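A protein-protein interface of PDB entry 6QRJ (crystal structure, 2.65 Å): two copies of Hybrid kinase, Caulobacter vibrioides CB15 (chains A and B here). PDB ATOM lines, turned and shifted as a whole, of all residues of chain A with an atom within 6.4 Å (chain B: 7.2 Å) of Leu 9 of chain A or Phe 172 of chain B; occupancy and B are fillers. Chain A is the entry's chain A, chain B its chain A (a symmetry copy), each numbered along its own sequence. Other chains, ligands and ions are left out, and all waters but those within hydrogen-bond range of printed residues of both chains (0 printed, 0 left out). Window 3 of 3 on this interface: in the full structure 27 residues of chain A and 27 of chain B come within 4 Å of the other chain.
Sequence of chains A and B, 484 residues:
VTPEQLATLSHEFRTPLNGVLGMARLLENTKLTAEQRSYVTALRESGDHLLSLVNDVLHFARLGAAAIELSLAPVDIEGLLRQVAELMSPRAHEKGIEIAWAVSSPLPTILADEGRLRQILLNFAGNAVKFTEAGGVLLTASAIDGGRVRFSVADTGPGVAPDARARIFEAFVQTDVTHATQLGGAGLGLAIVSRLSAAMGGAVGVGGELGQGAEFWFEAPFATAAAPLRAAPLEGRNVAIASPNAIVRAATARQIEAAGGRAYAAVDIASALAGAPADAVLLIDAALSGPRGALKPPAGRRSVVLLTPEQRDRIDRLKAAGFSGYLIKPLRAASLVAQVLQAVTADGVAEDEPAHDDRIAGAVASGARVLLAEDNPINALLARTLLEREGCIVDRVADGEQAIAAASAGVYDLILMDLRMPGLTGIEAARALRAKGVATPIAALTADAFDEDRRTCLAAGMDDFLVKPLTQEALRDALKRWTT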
ATOM      1  N   VAL A   1      24.293 -20.344  16.442  1.00  0.00           N
ATOM      2  CA  VAL A   1      25.537 -20.334  17.203  1.00  0.00           C
ATOM      3  C   VAL A   1      26.066 -21.764  17.321  1.00  0.00           C
ATOM      4  O   VAL A   1      27.215 -21.926  16.898  1.00  0.00           O
ATOM      5  CB  VAL A   1      25.303 -19.706  18.553  1.00  0.00           C
ATOM      6  N   GLU A   4      23.203 -27.814  20.028  1.00  0.00           N
ATOM      7  CA  GLU A   4      22.837 -28.100  21.450  1.00  0.00           C
ATOM      8  C   GLU A   4      22.235 -26.815  22.068  1.00  0.00           C
ATOM      9  O   GLU A   4      21.155 -26.896  22.731  1.00  0.00           O
ATOM     10  CB  GLU A   4      24.052 -28.630  22.231  1.00  0.00           C
ATOM     11  CG  GLU A   4      24.745 -29.831  21.599  1.00  0.00           C
ATOM     12  CD  GLU A   4      26.164 -29.619  21.072  1.00  0.00           C
ATOM     13  OE1 GLU A   4      27.134 -29.647  21.887  1.00  0.00           O
ATOM     14  OE2 GLU A   4      26.311 -29.460  19.836  1.00  0.00           O
ATOM     15  N   GLN A   5      22.888 -25.665  21.831  1.00  0.00           N
ATOM     16  CA  GLN A   5      22.541 -24.336  22.405  1.00  0.00           C
ATOM     17  C   GLN A   5      21.184 -23.897  21.837  1.00  0.00           C
ATOM     18  O   GLN A   5      20.343 -23.372  22.590  1.00  0.00           O
ATOM     19  CB  GLN A   5      23.682 -23.342  22.148  1.00  0.00           C
ATOM     20  CG  GLN A   5      24.973 -23.695  22.893  1.00  0.00           C
ATOM     21  CD  GLN A   5      25.950 -22.544  23.020  1.00  0.00           C
ATOM     22  OE1 GLN A   5      25.973 -21.639  22.178  1.00  0.00           O
ATOM     23  NE2 GLN A   5      26.768 -22.571  24.073  1.00  0.00           N
ATOM     24  N   LEU A   6      20.954 -24.180  20.559  1.00  0.00           N
ATOM     25  CA  LEU A   6      19.691 -23.860  19.847  1.00  0.00           C
ATOM     26  C   LEU A   6      18.522 -24.740  20.329  1.00  0.00           C
ATOM     27  O   LEU A   6      17.397 -24.200  20.485  1.00  0.00           O
ATOM     28  CB  LEU A   6      19.954 -24.058  18.355  1.00  0.00           C
ATOM     29  CG  LEU A   6      19.282 -23.074  17.396  1.00  0.00           C
ATOM     30  CD1 LEU A   6      18.980 -21.712  18.020  1.00  0.00           C
ATOM     31  CD2 LEU A   6      20.185 -22.886  16.196  1.00  0.00           C
ATOM     32  N   ALA A   7      18.760 -26.037  20.552  1.00  0.00           N
ATOM     33  CA  ALA A   7      17.745 -27.030  20.995  1.00  0.00           C
ATOM     34  C   ALA A   7      17.059 -26.565  22.287  1.00  0.00           C
ATOM     35  O   ALA A   7      15.848 -26.850  22.425  1.00  0.00           O
ATOM     36  CB  ALA A   7      18.374 -28.392  21.176  1.00  0.00           C
ATOM     37  N   THR A   8      17.792 -25.892  23.193  1.00  0.00           N
ATOM     38  CA  THR A   8      17.253 -25.328  24.470  1.00  0.00           C
ATOM     39  C   THR A   8      16.762 -23.881  24.243  1.00  0.00           C
ATOM     40  O   THR A   8      15.757 -23.525  24.889  1.00  0.00           O
ATOM     41  CB  THR A   8      18.246 -25.494  25.637  1.00  0.00           C
ATOM     42  OG1 THR A   8      19.499 -24.929  25.251  1.00  0.00           O
ATOM     43  CG2 THR A   8      18.450 -26.938  26.057  1.00  0.00           C
ATOM     44  N   LEU A   9      17.410 -23.084  23.372  1.00  0.00           N
ATOM     45  CA  LEU A   9      16.923 -21.748  22.904  1.00  0.00           C
ATOM     46  C   LEU A   9      15.468 -21.902  22.411  1.00  0.00           C
ATOM     47  O   LEU A   9      14.585 -21.103  22.844  1.00  0.00           O
ATOM     48  CB  LEU A   9      17.863 -21.240  21.796  1.00  0.00           C
ATOM     49  CG  LEU A   9      18.065 -19.730  21.629  1.00  0.00           C
ATOM     50  CD1 LEU A   9      19.293 -19.465  20.772  1.00  0.00           C
ATOM     51  CD2 LEU A   9      16.861 -19.047  20.987  1.00  0.00           C
ATOM     52  N   SER A  10      15.198 -22.919  21.579  1.00  0.00           N
ATOM     53  CA  SER A  10      13.856 -23.201  21.005  1.00  0.00           C
ATOM     54  C   SER A  10      12.866 -23.478  22.140  1.00  0.00           C
ATOM     55  O   SER A  10      11.842 -22.765  22.209  1.00  0.00           O
ATOM     56  CB  SER A  10      13.889 -24.342  20.017  1.00  0.00           C
ATOM     57  OG  SER A  10      13.885 -25.583  20.695  1.00  0.00           O
ATOM     58  N   HIS A  11      13.158 -24.483  22.975  1.00  0.00           N
ATOM     59  CA  HIS A  11      12.389 -24.852  24.206  1.00  0.00           C
ATOM     60  C   HIS A  11      11.922 -23.563  24.911  1.00  0.00           C
ATOM     61  O   HIS A  11      10.690 -23.451  25.150  1.00  0.00           O
ATOM     62  CB  HIS A  11      13.229 -25.814  25.082  1.00  0.00           C
ATOM     63  CG  HIS A  11      12.621 -26.326  26.358  1.00  0.00           C
ATOM     64  ND1 HIS A  11      11.566 -25.707  27.019  1.00  0.00           N
ATOM     65  CD2 HIS A  11      12.983 -27.371  27.143  1.00  0.00           C
ATOM     66  CE1 HIS A  11      11.268 -26.379  28.112  1.00  0.00           C
ATOM     67  NE2 HIS A  11      12.126 -27.402  28.215  1.00  0.00           N
ATOM     68  N   GLU A  12      12.843 -22.599  25.124  1.00  0.00           N
ATOM     69  CA  GLU A  12      12.665 -21.346  25.930  1.00  0.00           C
ATOM     70  C   GLU A  12      11.830 -20.282  25.201  1.00  0.00           C
ATOM     71  O   GLU A  12      11.050 -19.602  25.889  1.00  0.00           O
ATOM     72  CB  GLU A  12      14.001 -20.694  26.320  1.00  0.00           C
ATOM     73  CG  GLU A  12      14.790 -21.432  27.402  1.00  0.00           C
ATOM     74  CD  GLU A  12      14.178 -21.607  28.790  1.00  0.00           C
ATOM     75  OE1 GLU A  12      14.513 -20.796  29.713  1.00  0.00           O
ATOM     76  OE2 GLU A  12      13.433 -22.605  28.975  1.00  0.00           O
ATOM     77  N   PHE A  13      11.999 -20.083  23.897  1.00  0.00           N
ATOM     78  CA  PHE A  13      11.012 -19.281  23.136  1.00  0.00           C
ATOM     79  C   PHE A  13       9.705 -20.062  23.097  1.00  0.00           C
ATOM     80  O   PHE A  13       8.694 -19.547  23.586  1.00  0.00           O
ATOM     81  CB  PHE A  13      11.551 -18.896  21.774  1.00  0.00           C
ATOM     82  CG  PHE A  13      12.450 -17.706  21.913  1.00  0.00           C
ATOM     83  CD1 PHE A  13      13.730 -17.851  22.427  1.00  0.00           C
ATOM     84  CD2 PHE A  13      11.985 -16.430  21.635  1.00  0.00           C
ATOM     85  CE1 PHE A  13      14.544 -16.747  22.611  1.00  0.00           C
ATOM     86  CE2 PHE A  13      12.801 -15.327  21.814  1.00  0.00           C
ATOM     87  CZ  PHE A  13      14.073 -15.487  22.309  1.00  0.00           C
ATOM     88  N   ARG A  14       9.733 -21.305  22.635  1.00  0.00           N
ATOM     89  CA  ARG A  14       8.469 -22.032  22.401  1.00  0.00           C
ATOM     90  C   ARG A  14       7.634 -22.159  23.669  1.00  0.00           C
ATOM     91  O   ARG A  14       6.443 -21.820  23.592  1.00  0.00           O
ATOM     92  CB  ARG A  14       8.716 -23.391  21.781  1.00  0.00           C
ATOM     93  CG  ARG A  14       8.614 -23.277  20.275  1.00  0.00           C
ATOM     94  CD  ARG A  14       8.235 -24.580  19.636  1.00  0.00           C
ATOM     95  NE  ARG A  14       9.390 -25.104  18.940  1.00  0.00           N
ATOM     96  CZ  ARG A  14       9.718 -24.783  17.693  1.00  0.00           C
ATOM     97  NH1 ARG A  14       8.983 -23.921  17.004  1.00  0.00           N
ATOM     98  NH2 ARG A  14      10.794 -25.315  17.142  1.00  0.00           N
ATOM     99  N   LEU A  58      13.873 -20.431  13.729  1.00  0.00           N
ATOM    100  CA  LEU A  58      14.566 -21.599  14.321  1.00  0.00           C
ATOM    101  C   LEU A  58      14.851 -22.596  13.220  1.00  0.00           C
ATOM    102  O   LEU A  58      15.872 -23.241  13.281  1.00  0.00           O
ATOM    103  CB  LEU A  58      13.714 -22.221  15.419  1.00  0.00           C
ATOM    104  CG  LEU A  58      13.507 -21.324  16.641  1.00  0.00           C
ATOM    105  CD1 LEU A  58      12.916 -22.126  17.781  1.00  0.00           C
ATOM    106  CD2 LEU A  58      14.795 -20.638  17.108  1.00  0.00           C
ATOM    107  N   LEU B  53      12.897 -12.620  27.521  1.00  0.00           N
ATOM    108  CA  LEU B  53      13.847 -13.357  26.632  1.00  0.00           C
ATOM    109  C   LEU B  53      14.123 -12.540  25.363  1.00  0.00           C
ATOM    110  O   LEU B  53      15.264 -12.528  24.870  1.00  0.00           O
ATOM    111  CB  LEU B  53      13.307 -14.739  26.269  1.00  0.00           C
ATOM    112  CG  LEU B  53      13.187 -15.701  27.449  1.00  0.00           C
ATOM    113  CD1 LEU B  53      12.148 -16.788  27.161  1.00  0.00           C
ATOM    114  CD2 LEU B  53      14.530 -16.321  27.844  1.00  0.00           C
ATOM    115  N   VAL B  57      17.753 -11.064  24.177  1.00  0.00           N
ATOM    116  CA  VAL B  57      18.371 -11.514  22.921  1.00  0.00           C
ATOM    117  C   VAL B  57      18.601 -10.320  21.992  1.00  0.00           C
ATOM    118  O   VAL B  57      19.590 -10.359  21.252  1.00  0.00           O
ATOM    119  CB  VAL B  57      17.462 -12.568  22.300  1.00  0.00           C
ATOM    120  CG1 VAL B  57      17.733 -12.714  20.804  1.00  0.00           C
ATOM    121  CG2 VAL B  57      17.587 -13.885  23.060  1.00  0.00           C
ATOM    122  N   PHE B  60      21.489  -8.164  23.479  1.00  0.00           N
ATOM    123  CA  PHE B  60      22.761  -8.843  23.214  1.00  0.00           C
ATOM    124  C   PHE B  60      23.193  -8.506  21.812  1.00  0.00           C
ATOM    125  O   PHE B  60      24.291  -7.982  21.629  1.00  0.00           O
ATOM    126  CB  PHE B  60      22.605 -10.343  23.295  1.00  0.00           C
ATOM    127  CG  PHE B  60      23.901 -11.010  23.002  1.00  0.00           C
ATOM    128  CD1 PHE B  60      25.040 -10.639  23.696  1.00  0.00           C
ATOM    129  CD2 PHE B  60      23.980 -12.001  22.049  1.00  0.00           C
ATOM    130  CE1 PHE B  60      26.248 -11.259  23.442  1.00  0.00           C
ATOM    131  CE2 PHE B  60      25.187 -12.623  21.788  1.00  0.00           C
ATOM    132  CZ  PHE B  60      26.318 -12.243  22.478  1.00  0.00           C
ATOM    133  N   ILE B 168      31.636 -19.414  31.012  1.00  0.00           N
ATOM    134  CA  ILE B 168      30.311 -18.881  31.445  1.00  0.00           C
ATOM    135  C   ILE B 168      30.045 -17.438  30.943  1.00  0.00           C
ATOM    136  O   ILE B 168      28.869 -17.009  31.055  1.00  0.00           O
ATOM    137  CB  ILE B 168      30.127 -19.040  32.978  1.00  0.00           C
ATOM    138  CG1 ILE B 168      31.254 -18.403  33.802  1.00  0.00           C
ATOM    139  CG2 ILE B 168      29.929 -20.507  33.347  1.00  0.00           C
ATOM    140  CD1 ILE B 168      30.988 -18.330  35.306  1.00  0.00           C
ATOM    141  N   PHE B 169      31.033 -16.694  30.416  1.00  0.00           N
ATOM    142  CA  PHE B 169      30.845 -15.302  29.895  1.00  0.00           C
ATOM    143  C   PHE B 169      30.440 -15.331  28.406  1.00  0.00           C
ATOM    144  O   PHE B 169      30.400 -14.268  27.738  1.00  0.00           O
ATOM    145  CB  PHE B 169      32.109 -14.448  30.094  1.00  0.00           C
ATOM    146  CG  PHE B 169      32.407 -14.053  31.516  1.00  0.00           C
ATOM    147  CD1 PHE B 169      32.039 -12.813  31.998  1.00  0.00           C
ATOM    148  CD2 PHE B 169      33.061 -14.919  32.371  1.00  0.00           C
ATOM    149  CE1 PHE B 169      32.294 -12.464  33.313  1.00  0.00           C
ATOM    150  CE2 PHE B 169      33.344 -14.552  33.679  1.00  0.00           C
ATOM    151  CZ  PHE B 169      32.956 -13.325  34.151  1.00  0.00           C
ATOM    152  N   GLU B 170      30.183 -16.526  27.875  1.00  0.00           N
ATOM    153  CA  GLU B 170      29.805 -16.729  26.450  1.00  0.00           C
ATOM    154  C   GLU B 170      28.275 -16.848  26.359  1.00  0.00           C
ATOM    155  O   GLU B 170      27.624 -17.078  27.398  1.00  0.00           O
ATOM    156  CB  GLU B 170      30.518 -17.955  25.864  1.00  0.00           C
ATOM    157  CG  GLU B 170      32.033 -17.829  25.823  1.00  0.00           C
ATOM    158  CD  GLU B 170      32.794 -19.139  25.644  1.00  0.00           C
ATOM    159  OE1 GLU B 170      33.695 -19.413  26.474  1.00  0.00           O
ATOM    160  OE2 GLU B 170      32.499 -19.888  24.671  1.00  0.00           O
ATOM    161  N   ALA B 171      27.726 -16.676  25.154  1.00  0.00           N
ATOM    162  CA  ALA B 171      26.275 -16.694  24.868  1.00  0.00           C
ATOM    163  C   ALA B 171      25.742 -18.122  24.962  1.00  0.00           C
ATOM    164  O   ALA B 171      26.342 -19.040  24.349  1.00  0.00           O
ATOM    165  CB  ALA B 171      26.026 -16.103  23.510  1.00  0.00           C
ATOM    166  N   PHE B 172      24.650 -18.276  25.707  1.00  0.00           N
ATOM    167  CA  PHE B 172      23.781 -19.480  25.748  1.00  0.00           C
ATOM    168  C   PHE B 172      24.510 -20.614  26.485  1.00  0.00           C
ATOM    169  O   PHE B 172      24.125 -21.801  26.290  1.00  0.00           O
ATOM    170  CB  PHE B 172      23.326 -19.873  24.335  1.00  0.00           C
ATOM    171  CG  PHE B 172      22.787 -18.739  23.496  1.00  0.00           C
ATOM    172  CD1 PHE B 172      21.565 -18.151  23.783  1.00  0.00           C
ATOM    173  CD2 PHE B 172      23.496 -18.266  22.400  1.00  0.00           C
ATOM    174  CE1 PHE B 172      21.080 -17.109  23.008  1.00  0.00           C
ATOM    175  CE2 PHE B 172      23.009 -17.223  21.629  1.00  0.00           C
ATOM    176  CZ  PHE B 172      21.805 -16.641  21.940  1.00  0.00           C
ATOM    177  N   VAL B 173      25.499 -20.263  27.327  1.00  0.00           N
ATOM    178  CA  VAL B 173      26.194 -21.208  28.259  1.00  0.00           C
ATOM    179  C   VAL B 173      25.571 -21.066  29.665  1.00  0.00           C
ATOM    180  O   VAL B 173      25.474 -19.897  30.147  1.00  0.00           O
ATOM    181  CB  VAL B 173      27.718 -20.991  28.249  1.00  0.00           C
ATOM    182  CG1 VAL B 173      28.299 -21.090  26.845  1.00  0.00           C
ATOM    183  CG2 VAL B 173      28.094 -19.674  28.904  1.00  0.00           C
ATOM    184  N   GLN B 174      25.219 -22.217  30.285  1.00  0.00           N
ATOM    185  CA  GLN B 174      24.179 -22.419  31.348  1.00  0.00           C
ATOM    186  C   GLN B 174      24.777 -23.192  32.558  1.00  0.00           C
ATOM    187  O   GLN B 174      26.029 -23.104  32.743  1.00  0.00           O
ATOM    188  CB  GLN B 174      22.955 -23.072  30.676  1.00  0.00           C
ATOM    189  CG  GLN B 174      23.083 -24.566  30.314  1.00  0.00           C
ATOM    190  CD  GLN B 174      23.814 -24.985  29.045  1.00  0.00           C
ATOM    191  OE1 GLN B 174      24.376 -24.186  28.296  1.00  0.00           O
ATOM    192  NE2 GLN B 174      23.827 -26.286  28.785  1.00  0.00           N
ATOM    193  N   GLY B 185      17.201 -18.063  31.592  1.00  0.00           N
ATOM    194  CA  GLY B 185      16.743 -18.980  30.530  1.00  0.00           C
ATOM    195  C   GLY B 185      17.610 -18.837  29.292  1.00  0.00           C
ATOM    196  O   GLY B 185      18.134 -19.848  28.769  1.00  0.00           O
ATOM    197  N   ALA B 186      17.782 -17.599  28.844  1.00  0.00           N
ATOM    198  CA  ALA B 186      18.625 -17.236  27.684  1.00  0.00           C
ATOM    199  C   ALA B 186      20.045 -17.730  27.953  1.00  0.00           C
ATOM    200  O   ALA B 186      20.638 -18.336  27.050  1.00  0.00           O
ATOM    201  CB  ALA B 186      18.596 -15.736  27.513  1.00  0.00           C
ATOM    202  N   GLY B 187      20.528 -17.483  29.177  1.00  0.00           N
ATOM    203  CA  GLY B 187      21.947 -17.613  29.528  1.00  0.00           C
ATOM    204  C   GLY B 187      22.747 -16.526  28.828  1.00  0.00           C
ATOM    205  O   GLY B 187      23.780 -16.849  28.168  1.00  0.00           O
ATOM    206  N   LEU B 188      22.266 -15.280  28.930  1.00  0.00           N
ATOM    207  CA  LEU B 188      22.899 -14.120  28.255  1.00  0.00           C
ATOM    208  C   LEU B 188      23.406 -13.079  29.253  1.00  0.00           C
ATOM    209  O   LEU B 188      24.201 -12.248  28.866  1.00  0.00           O
ATOM    210  CB  LEU B 188      21.884 -13.494  27.298  1.00  0.00           C
ATOM    211  CG  LEU B 188      22.119 -13.802  25.818  1.00  0.00           C
ATOM    212  CD1 LEU B 188      22.228 -15.289  25.564  1.00  0.00           C
ATOM    213  CD2 LEU B 188      21.005 -13.226  24.966  1.00  0.00           C
ATOM    214  N   ALA B 191      27.078 -12.778  29.128  1.00  0.00           N
ATOM    215  CA  ALA B 191      27.470 -12.387  27.741  1.00  0.00           C
ATOM    216  C   ALA B 191      27.307 -10.871  27.570  1.00  0.00           C
ATOM    217  O   ALA B 191      28.206 -10.225  27.033  1.00  0.00           O
ATOM    218  CB  ALA B 191      26.654 -13.114  26.724  1.00  0.00           C
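OE1 of Gln 5 of chain A lies close to O of Ala 171 of chain B (3.4 Å).
The backbone carbonyl oxygen (O) of Gln 5 of chain A is in hydrogen-bond range of the side-chain hydroxyl (OG1) of Thr 8 of chain A (3.2 Å).
The side-chain amide oxygen of Gln 174 of chain B lies close to the backbone carbonyl oxygen of Phe 172 of chain B.
The backbone carbonyl oxygen of Gly 187 of chain B lies within hydrogen-bond range of the backbone NH of Phe 172 of chain B (3.0 Å).
Among the printed residues, pairs that only touch across the chains: Gln 5 of chain A with Phe 172 of chain B, Gln 5 of chain A with Val 173 of chain B, Leu 9 of chain A with Phe 172 of chain B, Glu 12 of chain A with Leu 53 of chain B, Glu 12 of chain A with Gly 185 of chain B and Phe 13 of chain A with Val 57 of chain B.
Of chain B, only Phe 172 (3.7 Å) comes within 4 Å of Leu 9 of chain A.
Of chain A, only Gln 5 and Leu 9 come within 4 Å of Phe 172 of chain B.
Of the printed residues of chain B, Gln 5 of chain A touches Ala 171 (3.4 Å), Phe 172 (3.5 Å) and Val 173 (3.5 Å).
Printed residues of chain A within 4 Å of Gly 185 of chain B: Glu 12.
Printed residues of chain A within 4 Å of Ala 171 of chain B: Gln 5 (3.4 Å).
Of the printed residues of chain A, Val 173 of chain B touches Gln 5.
Gly 187 of chain B touches none of the printed residues of chain A.
Of the 13 printed residues of chain A, 4 touch a printed residue of chain B.
Along chain A the printed residues that touch a printed residue of chain B span positions 5 to 13.
Printed residues of chain B that touch a printed residue of chain A: Leu 53, Val 57, Ala 171, Phe 172, Val 173 and Gly 185.
Hydrophobic or aromatic side chains of chain B within 4 Å of the printed part of chain A: Leu 53, Val 57, Phe 172 and Val 173.
Along chain B the printed residues that touch a printed residue of chain A span positions 53 to 185.
No position is printed for both chains.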
